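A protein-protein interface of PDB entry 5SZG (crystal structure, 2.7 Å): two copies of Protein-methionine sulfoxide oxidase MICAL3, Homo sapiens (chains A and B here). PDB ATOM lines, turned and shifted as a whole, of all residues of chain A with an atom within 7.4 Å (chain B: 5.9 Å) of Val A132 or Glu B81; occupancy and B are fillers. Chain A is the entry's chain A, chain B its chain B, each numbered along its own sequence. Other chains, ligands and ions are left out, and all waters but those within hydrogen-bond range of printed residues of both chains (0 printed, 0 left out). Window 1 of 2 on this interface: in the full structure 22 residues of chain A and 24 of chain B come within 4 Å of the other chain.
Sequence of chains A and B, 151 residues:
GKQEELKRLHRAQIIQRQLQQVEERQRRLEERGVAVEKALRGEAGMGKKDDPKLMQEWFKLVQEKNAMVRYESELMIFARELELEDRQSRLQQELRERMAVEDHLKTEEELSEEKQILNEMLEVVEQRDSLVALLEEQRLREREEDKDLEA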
ATOM      1  N   ILE A  77     -12.686  14.183  16.256  1.00  0.00           N
ATOM      2  CA  ILE A  77     -14.089  13.938  16.481  1.00  0.00           C
ATOM      3  C   ILE A  77     -14.314  12.473  16.475  1.00  0.00           C
ATOM      4  O   ILE A  77     -14.929  11.924  17.407  1.00  0.00           O
ATOM      5  CB  ILE A  77     -15.028  14.582  15.437  1.00  0.00           C
ATOM      6  CG1 ILE A  77     -15.135  16.073  15.645  1.00  0.00           C
ATOM      7  CG2 ILE A  77     -16.462  13.989  15.497  1.00  0.00           C
ATOM      8  CD1 ILE A  77     -15.534  16.786  14.346  1.00  0.00           C
ATOM      9  N   GLU A  81     -15.687  10.125  19.601  1.00  0.00           N
ATOM     10  CA  GLU A  81     -16.905   9.332  19.364  1.00  0.00           C
ATOM     11  C   GLU A  81     -16.607   7.877  19.737  1.00  0.00           C
ATOM     12  O   GLU A  81     -17.402   7.243  20.456  1.00  0.00           O
ATOM     13  CB  GLU A  81     -17.443   9.496  17.934  1.00  0.00           C
ATOM     14  CG  GLU A  81     -18.757   8.809  17.597  1.00  0.00           C
ATOM     15  CD  GLU A  81     -18.680   7.290  17.415  1.00  0.00           C
ATOM     16  OE1 GLU A  81     -17.723   6.809  16.767  1.00  0.00           O
ATOM     17  OE2 GLU A  81     -19.612   6.578  17.905  1.00  0.00           O
ATOM     18  N   GLU A 126     -25.809  11.423  24.653  1.00  0.00           N
ATOM     19  CA  GLU A 126     -26.104  12.798  24.255  1.00  0.00           C
ATOM     20  C   GLU A 126     -24.861  13.441  23.703  1.00  0.00           C
ATOM     21  O   GLU A 126     -24.908  14.109  22.692  1.00  0.00           O
ATOM     22  CB  GLU A 126     -26.638  13.618  25.436  1.00  0.00           C
ATOM     23  N   GLN A 127     -23.742  13.245  24.376  1.00  0.00           N
ATOM     24  CA  GLN A 127     -22.487  13.762  23.892  1.00  0.00           C
ATOM     25  C   GLN A 127     -22.144  13.217  22.509  1.00  0.00           C
ATOM     26  O   GLN A 127     -21.643  13.928  21.666  1.00  0.00           O
ATOM     27  CB  GLN A 127     -21.349  13.393  24.848  1.00  0.00           C
ATOM     28  CG  GLN A 127     -21.289  14.178  26.123  1.00  0.00           C
ATOM     29  CD  GLN A 127     -20.134  13.746  27.017  1.00  0.00           C
ATOM     30  OE1 GLN A 127     -19.013  13.468  26.548  1.00  0.00           O
ATOM     31  NE2 GLN A 127     -20.395  13.682  28.319  1.00  0.00           N
ATOM     32  N   ARG A 128     -22.402  11.942  22.306  1.00  0.00           N
ATOM     33  CA  ARG A 128     -22.111  11.279  21.073  1.00  0.00           C
ATOM     34  C   ARG A 128     -22.934  11.889  19.955  1.00  0.00           C
ATOM     35  O   ARG A 128     -22.420  12.193  18.851  1.00  0.00           O
ATOM     36  CB  ARG A 128     -22.376   9.751  21.237  1.00  0.00           C
ATOM     37  CG  ARG A 128     -21.590   8.914  20.245  1.00  0.00           C
ATOM     38  CD  ARG A 128     -22.390   8.783  18.945  1.00  0.00           C
ATOM     39  NE  ARG A 128     -23.485   7.839  19.114  1.00  0.00           N
ATOM     40  CZ  ARG A 128     -23.422   6.529  18.924  1.00  0.00           C
ATOM     41  NH1 ARG A 128     -22.317   5.949  18.497  1.00  0.00           N
ATOM     42  NH2 ARG A 128     -24.495   5.781  19.187  1.00  0.00           N
ATOM     43  N   ASP A 129     -24.214  12.093  20.202  1.00  0.00           N
ATOM     44  CA  ASP A 129     -25.082  12.679  19.179  1.00  0.00           C
ATOM     45  C   ASP A 129     -24.689  14.131  18.868  1.00  0.00           C
ATOM     46  O   ASP A 129     -24.793  14.590  17.744  1.00  0.00           O
ATOM     47  CB  ASP A 129     -26.572  12.554  19.568  1.00  0.00           C
ATOM     48  CG  ASP A 129     -27.024  11.079  19.836  1.00  0.00           C
ATOM     49  OD1 ASP A 129     -26.350  10.100  19.387  1.00  0.00           O
ATOM     50  OD2 ASP A 129     -28.091  10.902  20.501  1.00  0.00           O
ATOM     51  N   SER A 130     -24.208  14.834  19.870  1.00  0.00           N
ATOM     52  CA  SER A 130     -23.713  16.178  19.701  1.00  0.00           C
ATOM     53  C   SER A 130     -22.473  16.234  18.759  1.00  0.00           C
ATOM     54  O   SER A 130     -22.424  17.088  17.844  1.00  0.00           O
ATOM     55  CB  SER A 130     -23.467  16.827  21.064  1.00  0.00           C
ATOM     56  OG  SER A 130     -22.571  17.909  20.952  1.00  0.00           O
ATOM     57  N   LEU A 131     -21.518  15.331  18.965  1.00  0.00           N
ATOM     58  CA  LEU A 131     -20.348  15.138  18.042  1.00  0.00           C
ATOM     59  C   LEU A 131     -20.709  14.672  16.596  1.00  0.00           C
ATOM     60  O   LEU A 131     -20.077  15.085  15.640  1.00  0.00           O
ATOM     61  CB  LEU A 131     -19.371  14.103  18.618  1.00  0.00           C
ATOM     62  CG  LEU A 131     -18.639  14.448  19.923  1.00  0.00           C
ATOM     63  CD1 LEU A 131     -17.882  13.239  20.407  1.00  0.00           C
ATOM     64  CD2 LEU A 131     -17.718  15.648  19.724  1.00  0.00           C
ATOM     65  N   VAL A 132     -21.750  13.852  16.436  1.00  0.00           N
ATOM     66  CA  VAL A 132     -22.228  13.491  15.118  1.00  0.00           C
ATOM     67  C   VAL A 132     -22.831  14.711  14.434  1.00  0.00           C
ATOM     68  O   VAL A 132     -22.543  14.949  13.252  1.00  0.00           O
ATOM     69  CB  VAL A 132     -23.220  12.346  15.160  1.00  0.00           C
ATOM     70  CG1 VAL A 132     -23.779  12.064  13.785  1.00  0.00           C
ATOM     71  CG2 VAL A 132     -22.540  11.093  15.694  1.00  0.00           C
ATOM     72  N   ALA A 133     -23.576  15.530  15.185  1.00  0.00           N
ATOM     73  CA  ALA A 133     -24.158  16.795  14.636  1.00  0.00           C
ATOM     74  C   ALA A 133     -23.122  17.809  14.193  1.00  0.00           C
ATOM     75  O   ALA A 133     -23.280  18.442  13.181  1.00  0.00           O
ATOM     76  CB  ALA A 133     -25.124  17.436  15.620  1.00  0.00           C
ATOM     77  N   LEU A 134     -22.041  17.915  14.952  1.00  0.00           N
ATOM     78  CA  LEU A 134     -20.928  18.758  14.615  1.00  0.00           C
ATOM     79  C   LEU A 134     -20.198  18.258  13.344  1.00  0.00           C
ATOM     80  O   LEU A 134     -19.761  19.010  12.534  1.00  0.00           O
ATOM     81  CB  LEU A 134     -19.965  18.794  15.815  1.00  0.00           C
ATOM     82  CG  LEU A 134     -18.642  19.555  15.667  1.00  0.00           C
ATOM     83  CD1 LEU A 134     -18.814  20.971  15.088  1.00  0.00           C
ATOM     84  CD2 LEU A 134     -17.937  19.539  17.026  1.00  0.00           C
ATOM     85  N   LEU A 135     -20.006  16.967  13.251  1.00  0.00           N
ATOM     86  CA  LEU A 135     -19.313  16.378  12.119  1.00  0.00           C
ATOM     87  C   LEU A 135     -20.153  16.520  10.855  1.00  0.00           C
ATOM     88  O   LEU A 135     -19.625  16.744   9.792  1.00  0.00           O
ATOM     89  CB  LEU A 135     -19.045  14.907  12.436  1.00  0.00           C
ATOM     90  CG  LEU A 135     -18.406  14.007  11.439  1.00  0.00           C
ATOM     91  CD1 LEU A 135     -17.045  14.549  11.068  1.00  0.00           C
ATOM     92  CD2 LEU A 135     -18.345  12.591  12.020  1.00  0.00           C
ATOM     93  N   GLU A 136     -21.460  16.383  11.007  1.00  0.00           N
ATOM     94  CA  GLU A 136     -22.447  16.568   9.940  1.00  0.00           C
ATOM     95  C   GLU A 136     -22.338  18.015   9.445  1.00  0.00           C
ATOM     96  O   GLU A 136     -22.107  18.254   8.284  1.00  0.00           O
ATOM     97  CB  GLU A 136     -23.837  16.259  10.500  1.00  0.00           C
ATOM     98  CG  GLU A 136     -25.030  16.341   9.537  1.00  0.00           C
ATOM     99  CD  GLU A 136     -26.351  16.281  10.272  1.00  0.00           C
ATOM    100  OE1 GLU A 136     -27.049  17.318  10.294  1.00  0.00           O
ATOM    101  OE2 GLU A 136     -26.697  15.220  10.884  1.00  0.00           O
ATOM    102  N   GLU A 137     -22.396  18.971  10.350  1.00  0.00           N
ATOM    103  CA  GLU A 137     -22.212  20.392  10.004  1.00  0.00           C
ATOM    104  C   GLU A 137     -20.917  20.609   9.195  1.00  0.00           C
ATOM    105  O   GLU A 137     -20.960  21.158   8.093  1.00  0.00           O
ATOM    106  CB  GLU A 137     -22.201  21.244  11.276  1.00  0.00           C
ATOM    107  CG  GLU A 137     -22.351  22.752  11.023  1.00  0.00           C
ATOM    108  CD  GLU A 137     -22.130  23.677  12.228  1.00  0.00           C
ATOM    109  OE1 GLU A 137     -22.079  24.903  11.970  1.00  0.00           O
ATOM    110  OE2 GLU A 137     -22.004  23.231  13.404  1.00  0.00           O
ATOM    111  N   GLN A 138     -19.796  20.120   9.715  1.00  0.00           N
ATOM    112  CA  GLN A 138     -18.491  20.227   9.023  1.00  0.00           C
ATOM    113  C   GLN A 138     -18.470  19.612   7.611  1.00  0.00           C
ATOM    114  O   GLN A 138     -17.889  20.196   6.716  1.00  0.00           O
ATOM    115  CB  GLN A 138     -17.332  19.612   9.860  1.00  0.00           C
ATOM    116  CG  GLN A 138     -16.641  20.582  10.812  1.00  0.00           C
ATOM    117  CD  GLN A 138     -15.470  19.986  11.615  1.00  0.00           C
ATOM    118  OE1 GLN A 138     -14.818  19.023  11.193  1.00  0.00           O
ATOM    119  NE2 GLN A 138     -15.178  20.603  12.769  1.00  0.00           N
ATOM    120  N   ARG B  11     -32.168  20.301  10.537  1.00  0.00           N
ATOM    121  CA  ARG B  11     -31.075  19.479  10.010  1.00  0.00           C
ATOM    122  C   ARG B  11     -31.585  18.500   8.976  1.00  0.00           C
ATOM    123  O   ARG B  11     -30.940  18.278   7.971  1.00  0.00           O
ATOM    124  CB  ARG B  11     -30.364  18.698  11.133  1.00  0.00           C
ATOM    125  CG  ARG B  11     -29.919  19.578  12.298  1.00  0.00           C
ATOM    126  CD  ARG B  11     -28.567  19.230  12.873  1.00  0.00           C
ATOM    127  NE  ARG B  11     -28.275  17.797  12.954  1.00  0.00           N
ATOM    128  CZ  ARG B  11     -28.676  16.980  13.925  1.00  0.00           C
ATOM    129  NH1 ARG B  11     -29.457  17.414  14.928  1.00  0.00           N
ATOM    130  NH2 ARG B  11     -28.295  15.694  13.890  1.00  0.00           N
ATOM    131  N   MET B  76     -26.883  10.163   2.601  1.00  0.00           N
ATOM    132  CA  MET B  76     -27.664   8.988   2.979  1.00  0.00           C
ATOM    133  C   MET B  76     -27.438   8.601   4.429  1.00  0.00           C
ATOM    134  O   MET B  76     -28.416   8.353   5.180  1.00  0.00           O
ATOM    135  CB  MET B  76     -27.388   7.761   2.114  1.00  0.00           C
ATOM    136  CG  MET B  76     -27.687   7.935   0.618  1.00  0.00           C
ATOM    137  SD  MET B  76     -29.584   8.105   0.210  1.00  0.00           S
ATOM    138  CE  MET B  76     -30.010   6.163   0.285  1.00  0.00           C
ATOM    139  N   ILE B  77     -26.162   8.581   4.834  1.00  0.00           N
ATOM    140  CA  ILE B  77     -25.803   8.107   6.135  1.00  0.00           C
ATOM    141  C   ILE B  77     -26.288   9.077   7.187  1.00  0.00           C
ATOM    142  O   ILE B  77     -26.949   8.647   8.115  1.00  0.00           O
ATOM    143  CB  ILE B  77     -24.295   7.892   6.265  1.00  0.00           C
ATOM    144  CG1 ILE B  77     -23.886   6.639   5.496  1.00  0.00           C
ATOM    145  CG2 ILE B  77     -23.891   7.736   7.718  1.00  0.00           C
ATOM    146  CD1 ILE B  77     -22.441   6.690   5.091  1.00  0.00           C
ATOM    147  N   PHE B  78     -25.993  10.367   6.994  1.00  0.00           N
ATOM    148  CA  PHE B  78     -26.467  11.377   7.844  1.00  0.00           C
ATOM    149  C   PHE B  78     -27.969  11.375   8.052  1.00  0.00           C
ATOM    150  O   PHE B  78     -28.409  11.596   9.181  1.00  0.00           O
ATOM    151  CB  PHE B  78     -25.967  12.778   7.447  1.00  0.00           C
ATOM    152  CG  PHE B  78     -24.514  12.993   7.779  1.00  0.00           C
ATOM    153  CD1 PHE B  78     -24.053  12.840   9.089  1.00  0.00           C
ATOM    154  CD2 PHE B  78     -23.575  13.308   6.767  1.00  0.00           C
ATOM    155  CE1 PHE B  78     -22.712  13.004   9.390  1.00  0.00           C
ATOM    156  CE2 PHE B  78     -22.237  13.480   7.074  1.00  0.00           C
ATOM    157  CZ  PHE B  78     -21.808  13.314   8.386  1.00  0.00           C
ATOM    158  N   ALA B  79     -28.718  11.153   6.975  1.00  0.00           N
ATOM    159  CA  ALA B  79     -30.193  11.146   7.003  1.00  0.00           C
ATOM    160  C   ALA B  79     -30.728   9.983   7.788  1.00  0.00           C
ATOM    161  O   ALA B  79     -31.681  10.145   8.536  1.00  0.00           O
ATOM    162  CB  ALA B  79     -30.774  11.135   5.595  1.00  0.00           C
ATOM    163  N   ARG B  80     -30.132   8.806   7.641  1.00  0.00           N
ATOM    164  CA  ARG B  80     -30.545   7.643   8.447  1.00  0.00           C
ATOM    165  C   ARG B  80     -30.206   7.852   9.927  1.00  0.00           C
ATOM    166  O   ARG B  80     -31.030   7.619  10.804  1.00  0.00           O
ATOM    167  CB  ARG B  80     -29.862   6.397   7.925  1.00  0.00           C
ATOM    168  CG  ARG B  80     -30.223   5.113   8.615  1.00  0.00           C
ATOM    169  CD  ARG B  80     -31.577   4.600   8.188  1.00  0.00           C
ATOM    170  NE  ARG B  80     -31.691   3.183   8.558  1.00  0.00           N
ATOM    171  CZ  ARG B  80     -32.612   2.650   9.363  1.00  0.00           C
ATOM    172  NH1 ARG B  80     -33.584   3.396   9.907  1.00  0.00           N
ATOM    173  NH2 ARG B  80     -32.578   1.337   9.611  1.00  0.00           N
ATOM    174  N   GLU B  81     -28.980   8.279  10.190  1.00  0.00           N
ATOM    175  CA  GLU B  81     -28.512   8.597  11.517  1.00  0.00           C
ATOM    176  C   GLU B  81     -29.493   9.550  12.171  1.00  0.00           C
ATOM    177  O   GLU B  81     -29.885   9.346  13.337  1.00  0.00           O
ATOM    178  CB  GLU B  81     -27.080   9.181  11.457  1.00  0.00           C
ATOM    179  CG  GLU B  81     -26.616   9.864  12.753  1.00  0.00           C
ATOM    180  CD  GLU B  81     -27.056  11.354  12.926  1.00  0.00           C
ATOM    181  OE1 GLU B  81     -26.943  12.159  11.951  1.00  0.00           O
ATOM    182  OE2 GLU B  81     -27.505  11.740  14.048  1.00  0.00           O
ATOM    183  N   LEU B  82     -29.909  10.569  11.422  1.00  0.00           N
ATOM    184  CA  LEU B  82     -30.851  11.568  11.923  1.00  0.00           C
ATOM    185  C   LEU B  82     -32.237  10.979  12.289  1.00  0.00           C
ATOM    186  O   LEU B  82     -32.797  11.331  13.319  1.00  0.00           O
ATOM    187  CB  LEU B  82     -31.047  12.656  10.927  1.00  0.00           C
ATOM    188  CG  LEU B  82     -31.604  13.974  11.451  1.00  0.00           C
ATOM    189  CD1 LEU B  82     -31.038  14.535  12.738  1.00  0.00           C
ATOM    190  CD2 LEU B  82     -31.333  14.988  10.323  1.00  0.00           C
ATOM    191  N   GLU B  83     -32.791  10.129  11.425  1.00  0.00           N
ATOM    192  CA  GLU B  83     -33.984   9.366  11.786  1.00  0.00           C
ATOM    193  C   GLU B  83     -33.841   8.552  13.067  1.00  0.00           C
ATOM    194  O   GLU B  83     -34.764   8.517  13.885  1.00  0.00           O
ATOM    195  CB  GLU B  83     -34.430   8.412  10.684  1.00  0.00           C
ATOM    196  CG  GLU B  83     -35.897   8.099  10.728  1.00  0.00           C
ATOM    197  CD  GLU B  83     -36.776   9.353  10.727  1.00  0.00           C
ATOM    198  OE1 GLU B  83     -36.431  10.382  10.090  1.00  0.00           O
ATOM    199  OE2 GLU B  83     -37.816   9.333  11.399  1.00  0.00           O
ATOM    200  N   LEU B  84     -32.703   7.878  13.216  1.00  0.00           N
ATOM    201  CA  LEU B  84     -32.394   7.143  14.454  1.00  0.00           C
ATOM    202  C   LEU B  84     -32.235   8.069  15.681  1.00  0.00           C
ATOM    203  O   LEU B  84     -32.645   7.724  16.716  1.00  0.00           O
ATOM    204  CB  LEU B  84     -31.140   6.293  14.274  1.00  0.00           C
ATOM    205  CG  LEU B  84     -31.356   5.221  13.179  1.00  0.00           C
ATOM    206  CD1 LEU B  84     -30.047   4.566  12.744  1.00  0.00           C
ATOM    207  CD2 LEU B  84     -32.365   4.186  13.613  1.00  0.00           C
ATOM    208  N   GLU B  85     -31.596   9.212  15.553  1.00  0.00           N
ATOM    209  CA  GLU B  85     -31.530  10.182  16.602  1.00  0.00           C
ATOM    210  C   GLU B  85     -32.955  10.594  17.044  1.00  0.00           C
ATOM    211  O   GLU B  85     -33.210  10.856  18.233  1.00  0.00           O
ATOM    212  CB  GLU B  85     -30.756  11.450  16.123  1.00  0.00           C
ATOM    213  CG  GLU B  85     -30.179  12.288  17.259  1.00  0.00           C
ATOM    214  CD  GLU B  85     -29.471  13.585  16.772  1.00  0.00           C
ATOM    215  OE1 GLU B  85     -29.960  14.737  16.988  1.00  0.00           O
ATOM    216  OE2 GLU B  85     -28.377  13.446  16.164  1.00  0.00           O
ATOM    217  N   ASP B  86     -33.868  10.690  16.084  1.00  0.00           N
ATOM    218  CA  ASP B  86     -35.215  11.097  16.369  1.00  0.00           C
ATOM    219  C   ASP B  86     -35.918   9.986  17.128  1.00  0.00           C
ATOM    220  O   ASP B  86     -36.471  10.252  18.185  1.00  0.00           O
ATOM    221  CB  ASP B  86     -35.963  11.450  15.084  1.00  0.00           C
ATOM    222  CG  ASP B  86     -37.433  11.683  15.311  1.00  0.00           C
ATOM    223  OD1 ASP B  86     -37.753  12.719  15.920  1.00  0.00           O
ATOM    224  OD2 ASP B  86     -38.251  10.822  14.875  1.00  0.00           O
ATOM    225  N   ARG B 128     -26.855   3.159  15.232  1.00  0.00           N
ATOM    226  CA  ARG B 128     -26.191   4.429  15.033  1.00  0.00           C
ATOM    227  C   ARG B 128     -24.675   4.258  15.075  1.00  0.00           C
ATOM    228  O   ARG B 128     -24.010   4.781  14.188  1.00  0.00           O
ATOM    229  CB  ARG B 128     -26.641   5.494  16.032  1.00  0.00           C
ATOM    230  CG  ARG B 128     -28.021   5.964  15.769  1.00  0.00           C
ATOM    231  CD  ARG B 128     -28.635   6.943  16.740  1.00  0.00           C
ATOM    232  NE  ARG B 128     -28.253   8.293  16.350  1.00  0.00           N
ATOM    233  CZ  ARG B 128     -27.145   8.906  16.730  1.00  0.00           C
ATOM    234  NH1 ARG B 128     -26.287   8.324  17.563  1.00  0.00           N
ATOM    235  NH2 ARG B 128     -26.912  10.120  16.307  1.00  0.00           N
ATOM    236  N   LEU B 131     -23.613   2.854  11.636  1.00  0.00           N
ATOM    237  CA  LEU B 131     -23.541   3.949  10.635  1.00  0.00           C
ATOM    238  C   LEU B 131     -22.351   4.931  10.818  1.00  0.00           C
ATOM    239  O   LEU B 131     -21.815   5.439   9.861  1.00  0.00           O
ATOM    240  CB  LEU B 131     -24.833   4.736  10.627  1.00  0.00           C
ATOM    241  CG  LEU B 131     -26.074   3.984  10.172  1.00  0.00           C
ATOM    242  CD1 LEU B 131     -27.309   4.838  10.377  1.00  0.00           C
ATOM    243  CD2 LEU B 131     -25.931   3.572   8.703  1.00  0.00           C
ATOM    244  N   VAL B 132     -21.961   5.205  12.044  1.00  0.00           N
ATOM    245  CA  VAL B 132     -20.812   6.038  12.297  1.00  0.00           C
ATOM    246  C   VAL B 132     -19.559   5.315  11.832  1.00  0.00           C
ATOM    247  O   VAL B 132     -18.698   5.926  11.209  1.00  0.00           O
ATOM    248  CB  VAL B 132     -20.715   6.462  13.780  1.00  0.00           C
ATOM    249  CG1 VAL B 132     -19.438   7.234  14.029  1.00  0.00           C
ATOM    250  CG2 VAL B 132     -21.911   7.340  14.146  1.00  0.00           C
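Glu A81 touches Val B132 (OE1 to CG1, 3.3 Å).
Asp A129 touches Glu B85.
CD of Glu B81 touches CG1 of Val A132 (3.5 Å).
CB of Ala A133 touches CZ of Arg B11, at 3.96 Å.
Glu A136 touches Phe B78 (CA to CE1, 3.6 Å).
Of the printed residues of chain B, Val A132 touches Glu B81.
Glu B81 touches just these residues of chain A: Val A132 (3.5 Å) and Glu A136 (3.3 Å).
Of the printed residues of chain A, Glu B85 touches Asp A129 (3.95 Å).
Of the printed residues of chain A, Val B132 touches Glu A81.
The nearest residue of chain B that does not touch Val A132 is Val B132 (4.1 Å).
The nearest printed residue of chain B that does not touch Glu A136 is Leu B82 (4.7 Å).
Printed residues of chain A that touch a printed residue of chain B: Glu A81, Arg A128, Asp A129, Val A132, Ala A133 and Glu A136.
Hydrophobic or aromatic side chains of chain A within 4 Å of the printed part of chain B: Val A132 and Ala A133.
Of the 15 printed residues of chain B, 6 touch a printed residue of chain A.
Printed residues of chain B that touch a printed residue of chain A: Arg B11, Phe B78, Glu B81, Glu B85, Arg B128 and Val B132.
Hydrophobic or aromatic side chains of chain B that line the printed part of chain A: Phe B78 and Val B132.
Among the printed residues, Asp or Glu carboxylates within 4 Å of a Lys or Arg side-chain nitrogen of the other chain: Asp A129 with Arg B128 (2.5 Å) and Glu A136 with Arg B11 (3.0 Å).
The guanidinium group (NH1) of Arg B128 is in salt-bridge range of the side-chain carboxylate (OD1) of Asp A129 (2.5 Å).
The side-chain carboxylate of Glu A136 lies within salt-bridge range of the guanidinium group of Arg B11, 3.0 Å away.
The guanidinium group of Arg B128 lies close to the guanidinium group of Arg A128, at 3.2 Å.
The side-chain carboxylate (OE2) of Glu A136 sits close to the side-chain carboxylate (OE1) of Glu B81.
Glu A81 touches Val B132, and with the chains exchanged Val A132 touches Glu B81.
Arg A128 touches its own counterpart, Arg B128.
Positions printed for both chains: 77, 81, 128, 131 and 132.
Of the 9 pairs that touch across the chains among the printed residues, 3 have their exchanged pair printed and touching as well.
The side-chain carboxylate (OE2) of Glu A81 is in salt-bridge range of the guanidinium group (NH1) of Arg A128 (2.8 Å).
NE of Arg A128 is in salt-bridge range of OD1 of Asp A129, 3.7 Å away.
NH2 of Arg B11 lies within salt-bridge range of OE2 of Glu B85, at 3.2 Å.
The side-chain carboxylate (OE2) of Glu B81 is in salt-bridge range of the guanidinium group (NH2) of Arg B128.
NH2 of Arg B128 is in salt-bridge range of OE2 of Glu B85.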
